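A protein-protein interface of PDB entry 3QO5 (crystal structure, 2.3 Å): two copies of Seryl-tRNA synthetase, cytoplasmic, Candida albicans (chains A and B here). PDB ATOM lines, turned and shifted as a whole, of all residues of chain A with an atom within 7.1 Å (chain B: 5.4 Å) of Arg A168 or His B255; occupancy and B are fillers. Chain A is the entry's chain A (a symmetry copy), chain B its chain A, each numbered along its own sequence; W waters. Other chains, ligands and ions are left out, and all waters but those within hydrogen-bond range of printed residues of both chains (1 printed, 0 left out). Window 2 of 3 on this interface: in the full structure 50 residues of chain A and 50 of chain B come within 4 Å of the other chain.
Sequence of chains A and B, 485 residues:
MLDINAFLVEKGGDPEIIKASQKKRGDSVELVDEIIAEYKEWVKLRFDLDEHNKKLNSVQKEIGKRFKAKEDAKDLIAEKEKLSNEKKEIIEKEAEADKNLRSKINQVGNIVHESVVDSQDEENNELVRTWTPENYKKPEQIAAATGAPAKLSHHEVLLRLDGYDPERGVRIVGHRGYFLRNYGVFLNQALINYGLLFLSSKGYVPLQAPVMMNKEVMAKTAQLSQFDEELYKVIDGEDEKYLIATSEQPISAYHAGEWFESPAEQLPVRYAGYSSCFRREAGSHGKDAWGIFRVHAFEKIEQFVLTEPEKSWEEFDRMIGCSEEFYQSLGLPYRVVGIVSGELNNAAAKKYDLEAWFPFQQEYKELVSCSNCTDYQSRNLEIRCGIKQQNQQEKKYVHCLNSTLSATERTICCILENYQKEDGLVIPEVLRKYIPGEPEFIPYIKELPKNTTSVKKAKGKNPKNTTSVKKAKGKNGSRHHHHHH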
ATOM      1  N   ASP A 162      20.569 -41.314  13.997  1.00  0.00           N
ATOM      2  CA  ASP A 162      20.161 -40.083  13.360  1.00  0.00           C
ATOM      3  C   ASP A 162      20.073 -38.969  14.406  1.00  0.00           C
ATOM      4  O   ASP A 162      19.105 -38.228  14.462  1.00  0.00           O
ATOM      5  CB  ASP A 162      18.793 -40.239  12.693  1.00  0.00           C
ATOM      6  CG  ASP A 162      18.488 -39.095  11.733  1.00  0.00           C
ATOM      7  OD1 ASP A 162      19.443 -38.456  11.228  1.00  0.00           O
ATOM      8  OD2 ASP A 162      17.292 -38.825  11.505  1.00  0.00           O
ATOM      9  N   ASP A 165      23.971 -34.087  12.774  1.00  0.00           N
ATOM     10  CA  ASP A 165      24.270 -33.884  11.364  1.00  0.00           C
ATOM     11  C   ASP A 165      25.581 -33.156  11.164  1.00  0.00           C
ATOM     12  O   ASP A 165      25.612 -31.938  11.124  1.00  0.00           O
ATOM     13  CB  ASP A 165      23.174 -33.073  10.693  1.00  0.00           C
ATOM     14  CG  ASP A 165      23.098 -33.345   9.208  1.00  0.00           C
ATOM     15  OD1 ASP A 165      24.187 -33.481   8.579  1.00  0.00           O
ATOM     16  OD2 ASP A 165      21.965 -33.383   8.674  1.00  0.00           O
ATOM     17  N   PRO A 166      26.678 -33.906  11.032  1.00  0.00           N
ATOM     18  CA  PRO A 166      27.983 -33.281  10.794  1.00  0.00           C
ATOM     19  C   PRO A 166      28.165 -32.785   9.368  1.00  0.00           C
ATOM     20  O   PRO A 166      28.937 -31.869   9.136  1.00  0.00           O
ATOM     21  CB  PRO A 166      28.974 -34.411  11.085  1.00  0.00           C
ATOM     22  CG  PRO A 166      28.198 -35.673  10.787  1.00  0.00           C
ATOM     23  CD  PRO A 166      26.765 -35.367  11.194  1.00  0.00           C
ATOM     24  N   GLU A 167      27.505 -33.422   8.417  1.00  0.00           N
ATOM     25  CA  GLU A 167      27.687 -33.064   7.022  1.00  0.00           C
ATOM     26  C   GLU A 167      27.059 -31.677   6.688  1.00  0.00           C
ATOM     27  O   GLU A 167      27.718 -30.797   6.126  1.00  0.00           O
ATOM     28  CB  GLU A 167      27.139 -34.221   6.179  1.00  0.00           C
ATOM     29  CG  GLU A 167      27.078 -34.024   4.690  1.00  0.00           C
ATOM     30  CD  GLU A 167      26.851 -35.353   3.967  1.00  0.00           C
ATOM     31  OE1 GLU A 167      26.615 -35.334   2.735  1.00  0.00           O
ATOM     32  OE2 GLU A 167      26.938 -36.419   4.637  1.00  0.00           O
ATOM     33  N   ARG A 168      25.800 -31.475   7.045  1.00  0.00           N
ATOM     34  CA  ARG A 168      25.170 -30.167   6.868  1.00  0.00           C
ATOM     35  C   ARG A 168      25.820 -29.165   7.818  1.00  0.00           C
ATOM     36  O   ARG A 168      25.941 -27.978   7.511  1.00  0.00           O
ATOM     37  CB  ARG A 168      23.665 -30.258   7.095  1.00  0.00           C
ATOM     38  CG  ARG A 168      23.009 -31.192   6.099  1.00  0.00           C
ATOM     39  CD  ARG A 168      21.518 -31.237   6.302  1.00  0.00           C
ATOM     40  NE  ARG A 168      20.841 -31.895   5.194  1.00  0.00           N
ATOM     41  CZ  ARG A 168      20.427 -33.160   5.201  1.00  0.00           C
ATOM     42  NH1 ARG A 168      20.714 -33.965   6.234  1.00  0.00           N
ATOM     43  NH2 ARG A 168      19.786 -33.641   4.135  1.00  0.00           N
ATOM     44  N   GLY A 169      26.264 -29.662   8.967  1.00  0.00           N
ATOM     45  CA  GLY A 169      26.951 -28.842   9.942  1.00  0.00           C
ATOM     46  C   GLY A 169      28.212 -28.249   9.353  1.00  0.00           C
ATOM     47  O   GLY A 169      28.507 -27.073   9.538  1.00  0.00           O
ATOM     48  N   VAL A 170      29.014 -29.096   8.723  1.00  0.00           N
ATOM     49  CA  VAL A 170      30.256 -28.646   8.117  1.00  0.00           C
ATOM     50  C   VAL A 170      29.999 -27.624   7.004  1.00  0.00           C
ATOM     51  O   VAL A 170      30.765 -26.692   6.816  1.00  0.00           O
ATOM     52  CB  VAL A 170      31.063 -29.863   7.621  1.00  0.00           C
ATOM     53  CG1 VAL A 170      32.171 -29.458   6.645  1.00  0.00           C
ATOM     54  CG2 VAL A 170      31.604 -30.626   8.823  1.00  0.00           C
ATOM     55  N   ARG A 171      28.958 -27.847   6.216  1.00  0.00           N
ATOM     56  CA  ARG A 171      28.617 -26.929   5.130  1.00  0.00           C
ATOM     57  C   ARG A 171      28.274 -25.520   5.643  1.00  0.00           C
ATOM     58  O   ARG A 171      28.670 -24.499   5.070  1.00  0.00           O
ATOM     59  CB  ARG A 171      27.439 -27.466   4.315  1.00  0.00           C
ATOM     60  CG  ARG A 171      27.172 -26.623   3.071  1.00  0.00           C
ATOM     61  CD  ARG A 171      26.213 -27.309   2.104  1.00  0.00           C
ATOM     62  NE  ARG A 171      25.074 -27.949   2.760  1.00  0.00           N
ATOM     63  CZ  ARG A 171      24.059 -27.282   3.321  1.00  0.00           C
ATOM     64  NH1 ARG A 171      24.021 -25.940   3.303  1.00  0.00           N
ATOM     65  NH2 ARG A 171      23.073 -27.961   3.894  1.00  0.00           N
ATOM     66  N   ILE A 172      27.532 -25.484   6.744  1.00  0.00           N
ATOM     67  CA  ILE A 172      27.019 -24.224   7.259  1.00  0.00           C
ATOM     68  C   ILE A 172      28.004 -23.425   8.127  1.00  0.00           C
ATOM     69  O   ILE A 172      28.057 -22.185   8.025  1.00  0.00           O
ATOM     70  CB  ILE A 172      25.649 -24.469   7.939  1.00  0.00           C
ATOM     71  CG1 ILE A 172      24.600 -24.729   6.859  1.00  0.00           C
ATOM     72  CG2 ILE A 172      25.251 -23.333   8.860  1.00  0.00           C
ATOM     73  CD1 ILE A 172      23.505 -25.636   7.298  1.00  0.00           C
ATOM     74  N   VAL A 173      28.828 -24.111   8.922  1.00  0.00           N
ATOM     75  CA  VAL A 173      29.747 -23.386   9.814  1.00  0.00           C
ATOM     76  C   VAL A 173      31.204 -23.822   9.746  1.00  0.00           C
ATOM     77  O   VAL A 173      32.072 -23.206  10.362  1.00  0.00           O
ATOM     78  CB  VAL A 173      29.258 -23.436  11.291  1.00  0.00           C
ATOM     79  CG1 VAL A 173      29.197 -24.837  11.776  1.00  0.00           C
ATOM     80  CG2 VAL A 173      30.167 -22.611  12.197  1.00  0.00           C
ATOM     81  N   GLY A 174      31.467 -24.806   8.899  1.00  0.00           N
ATOM     82  CA  GLY A 174      32.794 -25.327   8.616  1.00  0.00           C
ATOM     83  C   GLY A 174      33.249 -26.419   9.576  1.00  0.00           C
ATOM     84  O   GLY A 174      32.434 -27.108  10.192  1.00  0.00           O
ATOM     85  N   GLY A 177      31.590 -28.453  12.587  1.00  0.00           N
ATOM     86  CA  GLY A 177      30.275 -27.872  12.804  1.00  0.00           C
ATOM     87  C   GLY A 177      29.257 -28.995  12.866  1.00  0.00           C
ATOM     88  O   GLY A 177      29.399 -29.985  12.179  1.00  0.00           O
ATOM     89  N   TYR A 178      28.182 -28.831  13.618  1.00  0.00           N
ATOM     90  CA  TYR A 178      27.191 -29.912  13.680  1.00  0.00           C
ATOM     91  C   TYR A 178      25.842 -29.397  14.102  1.00  0.00           C
ATOM     92  O   TYR A 178      25.757 -28.410  14.853  1.00  0.00           O
ATOM     93  CB  TYR A 178      27.647 -31.029  14.623  1.00  0.00           C
ATOM     94  CG  TYR A 178      27.722 -30.567  16.055  1.00  0.00           C
ATOM     95  CD1 TYR A 178      26.678 -30.793  16.957  1.00  0.00           C
ATOM     96  CD2 TYR A 178      28.847 -29.882  16.506  1.00  0.00           C
ATOM     97  CE1 TYR A 178      26.776 -30.365  18.289  1.00  0.00           C
ATOM     98  CE2 TYR A 178      28.945 -29.439  17.809  1.00  0.00           C
ATOM     99  CZ  TYR A 178      27.921 -29.686  18.699  1.00  0.00           C
ATOM    100  OH  TYR A 178      28.063 -29.238  19.983  1.00  0.00           O
ATOM    101  N   PHE A 179      24.786 -30.058  13.629  1.00  0.00           N
ATOM    102  CA  PHE A 179      23.481 -29.886  14.257  1.00  0.00           C
ATOM    103  C   PHE A 179      23.267 -31.110  15.128  1.00  0.00           C
ATOM    104  O   PHE A 179      23.731 -32.199  14.806  1.00  0.00           O
ATOM    105  CB  PHE A 179      22.389 -29.923  13.177  1.00  0.00           C
ATOM    106  CG  PHE A 179      22.389 -28.736  12.240  1.00  0.00           C
ATOM    107  CD1 PHE A 179      21.351 -27.796  12.275  1.00  0.00           C
ATOM    108  CD2 PHE A 179      23.401 -28.585  11.283  1.00  0.00           C
ATOM    109  CE1 PHE A 179      21.336 -26.719  11.400  1.00  0.00           C
ATOM    110  CE2 PHE A 179      23.403 -27.507  10.400  1.00  0.00           C
ATOM    111  CZ  PHE A 179      22.357 -26.557  10.465  1.00  0.00           C
ATOM    112  N   ARG A 181      20.094 -33.566  16.387  1.00  0.00           N
ATOM    113  CA  ARG A 181      18.827 -33.918  15.780  1.00  0.00           C
ATOM    114  C   ARG A 181      18.104 -34.821  16.707  1.00  0.00           C
ATOM    115  O   ARG A 181      18.692 -35.709  17.303  1.00  0.00           O
ATOM    116  CB  ARG A 181      19.054 -34.604  14.448  1.00  0.00           C
ATOM    117  CG  ARG A 181      19.471 -33.759  13.302  1.00  0.00           C
ATOM    118  CD  ARG A 181      19.514 -34.630  12.032  1.00  0.00           C
ATOM    119  NE  ARG A 181      18.375 -35.529  11.876  1.00  0.00           N
ATOM    120  CZ  ARG A 181      17.308 -35.299  11.124  1.00  0.00           C
ATOM    121  NH1 ARG A 181      17.235 -34.219  10.344  1.00  0.00           N
ATOM    122  NH2 ARG A 181      16.335 -36.200  11.111  1.00  0.00           N
ATOM    123  N   LYS A 446      19.381 -45.709  11.070  1.00  0.00           N
ATOM    124  CA  LYS A 446      20.181 -45.673   9.853  1.00  0.00           C
ATOM    125  C   LYS A 446      21.267 -46.737   9.951  1.00  0.00           C
ATOM    126  O   LYS A 446      21.783 -47.006  11.036  1.00  0.00           O
ATOM    127  CB  LYS A 446      20.847 -44.309   9.685  1.00  0.00           C
ATOM    128  CG  LYS A 446      19.899 -43.250   9.147  1.00  0.00           C
ATOM    129  CD  LYS A 446      20.604 -41.941   8.842  1.00  0.00           C
ATOM    130  CE  LYS A 446      21.012 -41.206  10.119  1.00  0.00           C
ATOM    131  NZ  LYS A 446      21.559 -39.831   9.869  1.00  0.00           N
ATOM    132  N   ILE B 251      18.986 -23.090   9.848  1.00  0.00           N
ATOM    133  CA  ILE B 251      18.043 -24.137   9.508  1.00  0.00           C
ATOM    134  C   ILE B 251      17.471 -23.913   8.099  1.00  0.00           C
ATOM    135  O   ILE B 251      17.121 -24.881   7.395  1.00  0.00           O
ATOM    136  CB  ILE B 251      16.950 -24.255  10.589  1.00  0.00           C
ATOM    137  CG1 ILE B 251      17.543 -24.736  11.928  1.00  0.00           C
ATOM    138  CG2 ILE B 251      15.845 -25.181  10.135  1.00  0.00           C
ATOM    139  CD1 ILE B 251      16.528 -24.766  13.073  1.00  0.00           C
ATOM    140  N   SER B 252      17.330 -22.654   7.678  1.00  0.00           N
ATOM    141  CA  SER B 252      16.832 -22.396   6.323  1.00  0.00           C
ATOM    142  C   SER B 252      17.814 -22.965   5.314  1.00  0.00           C
ATOM    143  O   SER B 252      17.427 -23.397   4.238  1.00  0.00           O
ATOM    144  CB  SER B 252      16.579 -20.905   6.022  1.00  0.00           C
ATOM    145  OG  SER B 252      17.775 -20.158   5.999  1.00  0.00           O
ATOM    146  N   ALA B 253      19.091 -22.986   5.674  1.00  0.00           N
ATOM    147  CA  ALA B 253      20.116 -23.473   4.757  1.00  0.00           C
ATOM    148  C   ALA B 253      20.384 -24.965   4.894  1.00  0.00           C
ATOM    149  O   ALA B 253      21.174 -25.536   4.139  1.00  0.00           O
ATOM    150  CB  ALA B 253      21.393 -22.686   4.934  1.00  0.00           C
ATOM    151  N   TYR B 254      19.715 -25.585   5.863  1.00  0.00           N
ATOM    152  CA  TYR B 254      19.922 -26.997   6.150  1.00  0.00           C
ATOM    153  C   TYR B 254      19.771 -27.865   4.879  1.00  0.00           C
ATOM    154  O   TYR B 254      20.565 -28.772   4.644  1.00  0.00           O
ATOM    155  CB  TYR B 254      18.908 -27.414   7.233  1.00  0.00           C
ATOM    156  CG  TYR B 254      19.091 -28.791   7.853  1.00  0.00           C
ATOM    157  CD1 TYR B 254      20.135 -29.053   8.742  1.00  0.00           C
ATOM    158  CD2 TYR B 254      18.169 -29.804   7.618  1.00  0.00           C
ATOM    159  CE1 TYR B 254      20.285 -30.318   9.345  1.00  0.00           C
ATOM    160  CE2 TYR B 254      18.301 -31.053   8.202  1.00  0.00           C
ATOM    161  CZ  TYR B 254      19.357 -31.306   9.062  1.00  0.00           C
ATOM    162  OH  TYR B 254      19.462 -32.552   9.610  1.00  0.00           O
ATOM    163  N   HIS B 255      18.759 -27.586   4.068  1.00  0.00           N
ATOM    164  CA  HIS B 255      18.520 -28.364   2.852  1.00  0.00           C
ATOM    165  C   HIS B 255      18.999 -27.643   1.598  1.00  0.00           C
ATOM    166  O   HIS B 255      18.481 -27.896   0.526  1.00  0.00           O
ATOM    167  CB  HIS B 255      17.041 -28.728   2.710  1.00  0.00           C
ATOM    168  CG  HIS B 255      16.585 -29.731   3.722  1.00  0.00           C
ATOM    169  ND1 HIS B 255      17.045 -31.036   3.736  1.00  0.00           N
ATOM    170  CD2 HIS B 255      15.776 -29.601   4.801  1.00  0.00           C
ATOM    171  CE1 HIS B 255      16.497 -31.681   4.749  1.00  0.00           C
ATOM    172  NE2 HIS B 255      15.739 -30.826   5.424  1.00  0.00           N
ATOM    173  N   ALA B 256      19.878 -26.656   1.739  1.00  0.00           N
ATOM    174  CA  ALA B 256      20.375 -25.944   0.559  1.00  0.00           C
ATOM    175  C   ALA B 256      20.899 -26.959  -0.455  1.00  0.00           C
ATOM    176  O   ALA B 256      21.523 -27.945  -0.065  1.00  0.00           O
ATOM    177  CB  ALA B 256      21.486 -24.974   0.944  1.00  0.00           C
ATOM    178  N   GLY B 257      20.597 -26.757  -1.739  1.00  0.00           N
ATOM    179  CA  GLY B 257      21.160 -27.590  -2.800  1.00  0.00           C
ATOM    180  C   GLY B 257      20.586 -28.998  -2.849  1.00  0.00           C
ATOM    181  O   GLY B 257      21.126 -29.888  -3.504  1.00  0.00           O
ATOM    182  N   GLU B 258      19.457 -29.187  -2.180  1.00  0.00           N
ATOM    183  CA  GLU B 258      18.807 -30.490  -2.162  1.00  0.00           C
ATOM    184  C   GLU B 258      17.517 -30.413  -2.958  1.00  0.00           C
ATOM    185  O   GLU B 258      17.143 -29.341  -3.431  1.00  0.00           O
ATOM    186  CB  GLU B 258      18.563 -30.991  -0.737  1.00  0.00           C
ATOM    187  CG  GLU B 258      19.827 -31.259   0.016  1.00  0.00           C
ATOM    188  CD  GLU B 258      19.566 -31.657   1.466  1.00  0.00           C
ATOM    189  OE1 GLU B 258      18.493 -32.238   1.745  1.00  0.00           O
ATOM    190  OE2 GLU B 258      20.430 -31.390   2.315  1.00  0.00           O
ATOM    191  N   PHE B 260      13.575 -32.042  -3.265  1.00  0.00           N
ATOM    192  CA  PHE B 260      12.467 -32.892  -2.878  1.00  0.00           C
ATOM    193  C   PHE B 260      11.742 -33.333  -4.141  1.00  0.00           C
ATOM    194  O   PHE B 260      10.785 -32.696  -4.589  1.00  0.00           O
ATOM    195  CB  PHE B 260      11.544 -32.160  -1.909  1.00  0.00           C
ATOM    196  CG  PHE B 260      12.219 -31.821  -0.620  1.00  0.00           C
ATOM    197  CD1 PHE B 260      12.245 -32.739   0.423  1.00  0.00           C
ATOM    198  CD2 PHE B 260      12.872 -30.604  -0.458  1.00  0.00           C
ATOM    199  CE1 PHE B 260      12.894 -32.431   1.631  1.00  0.00           C
ATOM    200  CE2 PHE B 260      13.528 -30.299   0.736  1.00  0.00           C
ATOM    201  CZ  PHE B 260      13.529 -31.206   1.783  1.00  0.00           C
ATOM    202  N   VAL B 269       8.240 -30.828   5.518  1.00  0.00           N
ATOM    203  CA  VAL B 269       9.248 -31.071   6.529  1.00  0.00           C
ATOM    204  C   VAL B 269       9.179 -29.964   7.612  1.00  0.00           C
ATOM    205  O   VAL B 269       9.202 -28.771   7.322  1.00  0.00           O
ATOM    206  CB  VAL B 269      10.652 -31.102   5.893  1.00  0.00           C
ATOM    207  CG1 VAL B 269      11.697 -30.827   6.913  1.00  0.00           C
ATOM    208  CG2 VAL B 269      10.898 -32.489   5.212  1.00  0.00           C
ATOM    209  N   TYR B 271      10.616 -28.460  11.295  1.00  0.00           N
ATOM    210  CA  TYR B 271      11.663 -28.459  12.303  1.00  0.00           C
ATOM    211  C   TYR B 271      11.331 -27.618  13.507  1.00  0.00           C
ATOM    212  O   TYR B 271      10.880 -26.486  13.398  1.00  0.00           O
ATOM    213  CB  TYR B 271      12.949 -27.918  11.703  1.00  0.00           C
ATOM    214  CG  TYR B 271      13.496 -28.831  10.663  1.00  0.00           C
ATOM    215  CD1 TYR B 271      13.947 -30.102  11.012  1.00  0.00           C
ATOM    216  CD2 TYR B 271      13.526 -28.466   9.331  1.00  0.00           C
ATOM    217  CE1 TYR B 271      14.449 -30.992  10.050  1.00  0.00           C
ATOM    218  CE2 TYR B 271      14.036 -29.323   8.369  1.00  0.00           C
ATOM    219  CZ  TYR B 271      14.493 -30.599   8.739  1.00  0.00           C
ATOM    220  OH  TYR B 271      14.978 -31.468   7.790  1.00  0.00           O
ATOM    221  N   LEU B 306       9.298 -26.530   5.488  1.00  0.00           N
ATOM    222  CA  LEU B 306       9.341 -26.540   4.035  1.00  0.00           C
ATOM    223  C   LEU B 306       8.093 -27.238   3.535  1.00  0.00           C
ATOM    224  O   LEU B 306       7.734 -28.298   4.043  1.00  0.00           O
ATOM    225  CB  LEU B 306      10.559 -27.299   3.527  1.00  0.00           C
ATOM    226  CG  LEU B 306      11.928 -26.799   3.982  1.00  0.00           C
ATOM    227  CD1 LEU B 306      13.052 -27.471   3.202  1.00  0.00           C
ATOM    228  CD2 LEU B 306      11.935 -25.327   3.709  1.00  0.00           C
ATOM    229  N   LEU B 381      18.844 -20.639  -2.186  1.00  0.00           N
ATOM    230  CA  LEU B 381      19.505 -21.789  -1.552  1.00  0.00           C
ATOM    231  C   LEU B 381      19.396 -23.039  -2.456  1.00  0.00           C
ATOM    232  O   LEU B 381      19.888 -24.112  -2.118  1.00  0.00           O
ATOM    233  CB  LEU B 381      18.861 -22.025  -0.183  1.00  0.00           C
ATOM    234  CG  LEU B 381      19.205 -20.902   0.815  1.00  0.00           C
ATOM    235  CD1 LEU B 381      18.221 -20.796   1.973  1.00  0.00           C
ATOM    236  CD2 LEU B 381      20.668 -20.985   1.317  1.00  0.00           C
ATOM    237  N   GLU B 382      18.743 -22.879  -3.605  1.00  0.00           N
ATOM    238  CA  GLU B 382      18.512 -23.973  -4.553  1.00  0.00           C
ATOM    239  C   GLU B 382      17.891 -25.207  -3.904  1.00  0.00           C
ATOM    240  O   GLU B 382      18.428 -26.308  -4.017  1.00  0.00           O
ATOM    241  CB  GLU B 382      19.832 -24.354  -5.251  1.00  0.00           C
ATOM    242  CG  GLU B 382      20.371 -23.307  -6.206  1.00  0.00           C
ATOM    243  CD  GLU B 382      19.539 -23.131  -7.449  1.00  0.00           C
ATOM    244  OE1 GLU B 382      18.688 -23.997  -7.745  1.00  0.00           O
ATOM    245  OE2 GLU B 382      19.742 -22.111  -8.135  1.00  0.00           O
ATOM    246  N   ILE B 383      16.742 -25.026  -3.259  1.00  0.00           N
ATOM    247  CA  ILE B 383      16.005 -26.137  -2.661  1.00  0.00           C
ATOM    248  C   ILE B 383      14.791 -26.466  -3.533  1.00  0.00           C
ATOM    249  O   ILE B 383      13.750 -25.852  -3.426  1.00  0.00           O
ATOM    250  CB  ILE B 383      15.550 -25.797  -1.235  1.00  0.00           C
ATOM    251  CG1 ILE B 383      16.718 -25.189  -0.439  1.00  0.00           C
ATOM    252  CG2 ILE B 383      14.961 -27.034  -0.564  1.00  0.00           C
ATOM    253  CD1 ILE B 383      16.410 -24.807   0.991  1.00  0.00           C
HETATM  254  O   HOH W   1      22.951 -30.605   1.877  1.00  0.00           O
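NH1 of Arg A168 is in salt-bridge range of OD2 of Asp A165, 2.8 Å away.
A ring nitrogen (NE2) of His B255 lies within hydrogen-bond range of the side-chain hydroxyl (OH) of Tyr B271, at 2.6 Å.
OD1 of Asp A165 is in hydrogen-bond range of N of Glu A167 (3.3 Å).
OD2 of Asp A162 is in salt-bridge range of NH2 of Arg A181.
A ring nitrogen (ND1) of His B255 lies within hydrogen-bond range of the side-chain carboxylate (OE1) of Glu B258.
The backbone carbonyl oxygen (O) of Phe A179 sits at hydrogen-bond distance from the backbone NH (N) of Asp A165 (2.8 Å).
Among the printed residues, 10 pairs touch across the chains.
Among the printed residues, Asp or Glu carboxylates within 4 Å of a Lys or Arg side-chain nitrogen of the other chain: Arg A168 with Glu B258.
Arg A168 touches three residues of chain B.
Of chain A, only Arg A168 (3.8 Å) comes within 4 Å of His B255.
Of the printed residues of chain A, Glu B258 touches Arg A168 (3.0 Å).
Printed residues of chain B within 4 Å of Arg A181: Tyr B254.
Printed residues of chain B within 4 Å of Phe A179: Tyr B254.
Printed residues of chain B within 4 Å of Arg A171: Ala B253, Tyr B254 and Ala B256.
Of the printed residues of chain A, Ala B256 touches Arg A171 (3.6 Å).
Glu A167 touches none of the printed residues of chain B.
Leu B381 touches none of the printed residues of chain A.
The nearest printed residue of chain B that does not touch Asp A165 is Glu B258 (6.8 Å).
Arg A168 touches His B255 (NH2 to ND1, 3.8 Å).
Ala B256 touches Arg A171.
Ala B253 touches Ile A172 (O to CD1, 3.9 Å).
Phe A179 touches Tyr B254.
Water W1 lies within hydrogen-bond range of the side-chain carboxylate of Glu B258 (2.7 Å) and the guanidinium group of Arg A171 (3.3 Å).
No position is printed for both chains.
The guanidinium group (NH2) of Arg A171 sits at hydrogen-bond distance from the backbone carbonyl oxygen (O) of Tyr B254, 2.7 Å away.
The backbone carbonyl oxygen (O) of Tyr B254 sits close to the guanidinium group (NE) of Arg A168 (3.2 Å).
OH of Tyr B254 sits at hydrogen-bond distance from OD2 of Asp A165.
The backbone carbonyl oxygen of Ala B253 is in hydrogen-bond range of the guanidinium group of Arg A171, at 3.0 Å.
The side-chain carboxylate (OE2) of Glu B258 lies within salt-bridge range of the guanidinium group (NE) of Arg A168 (3.0 Å).
OH of Tyr B254 sits at hydrogen-bond distance from NH1 of Arg A181 (2.9 Å).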
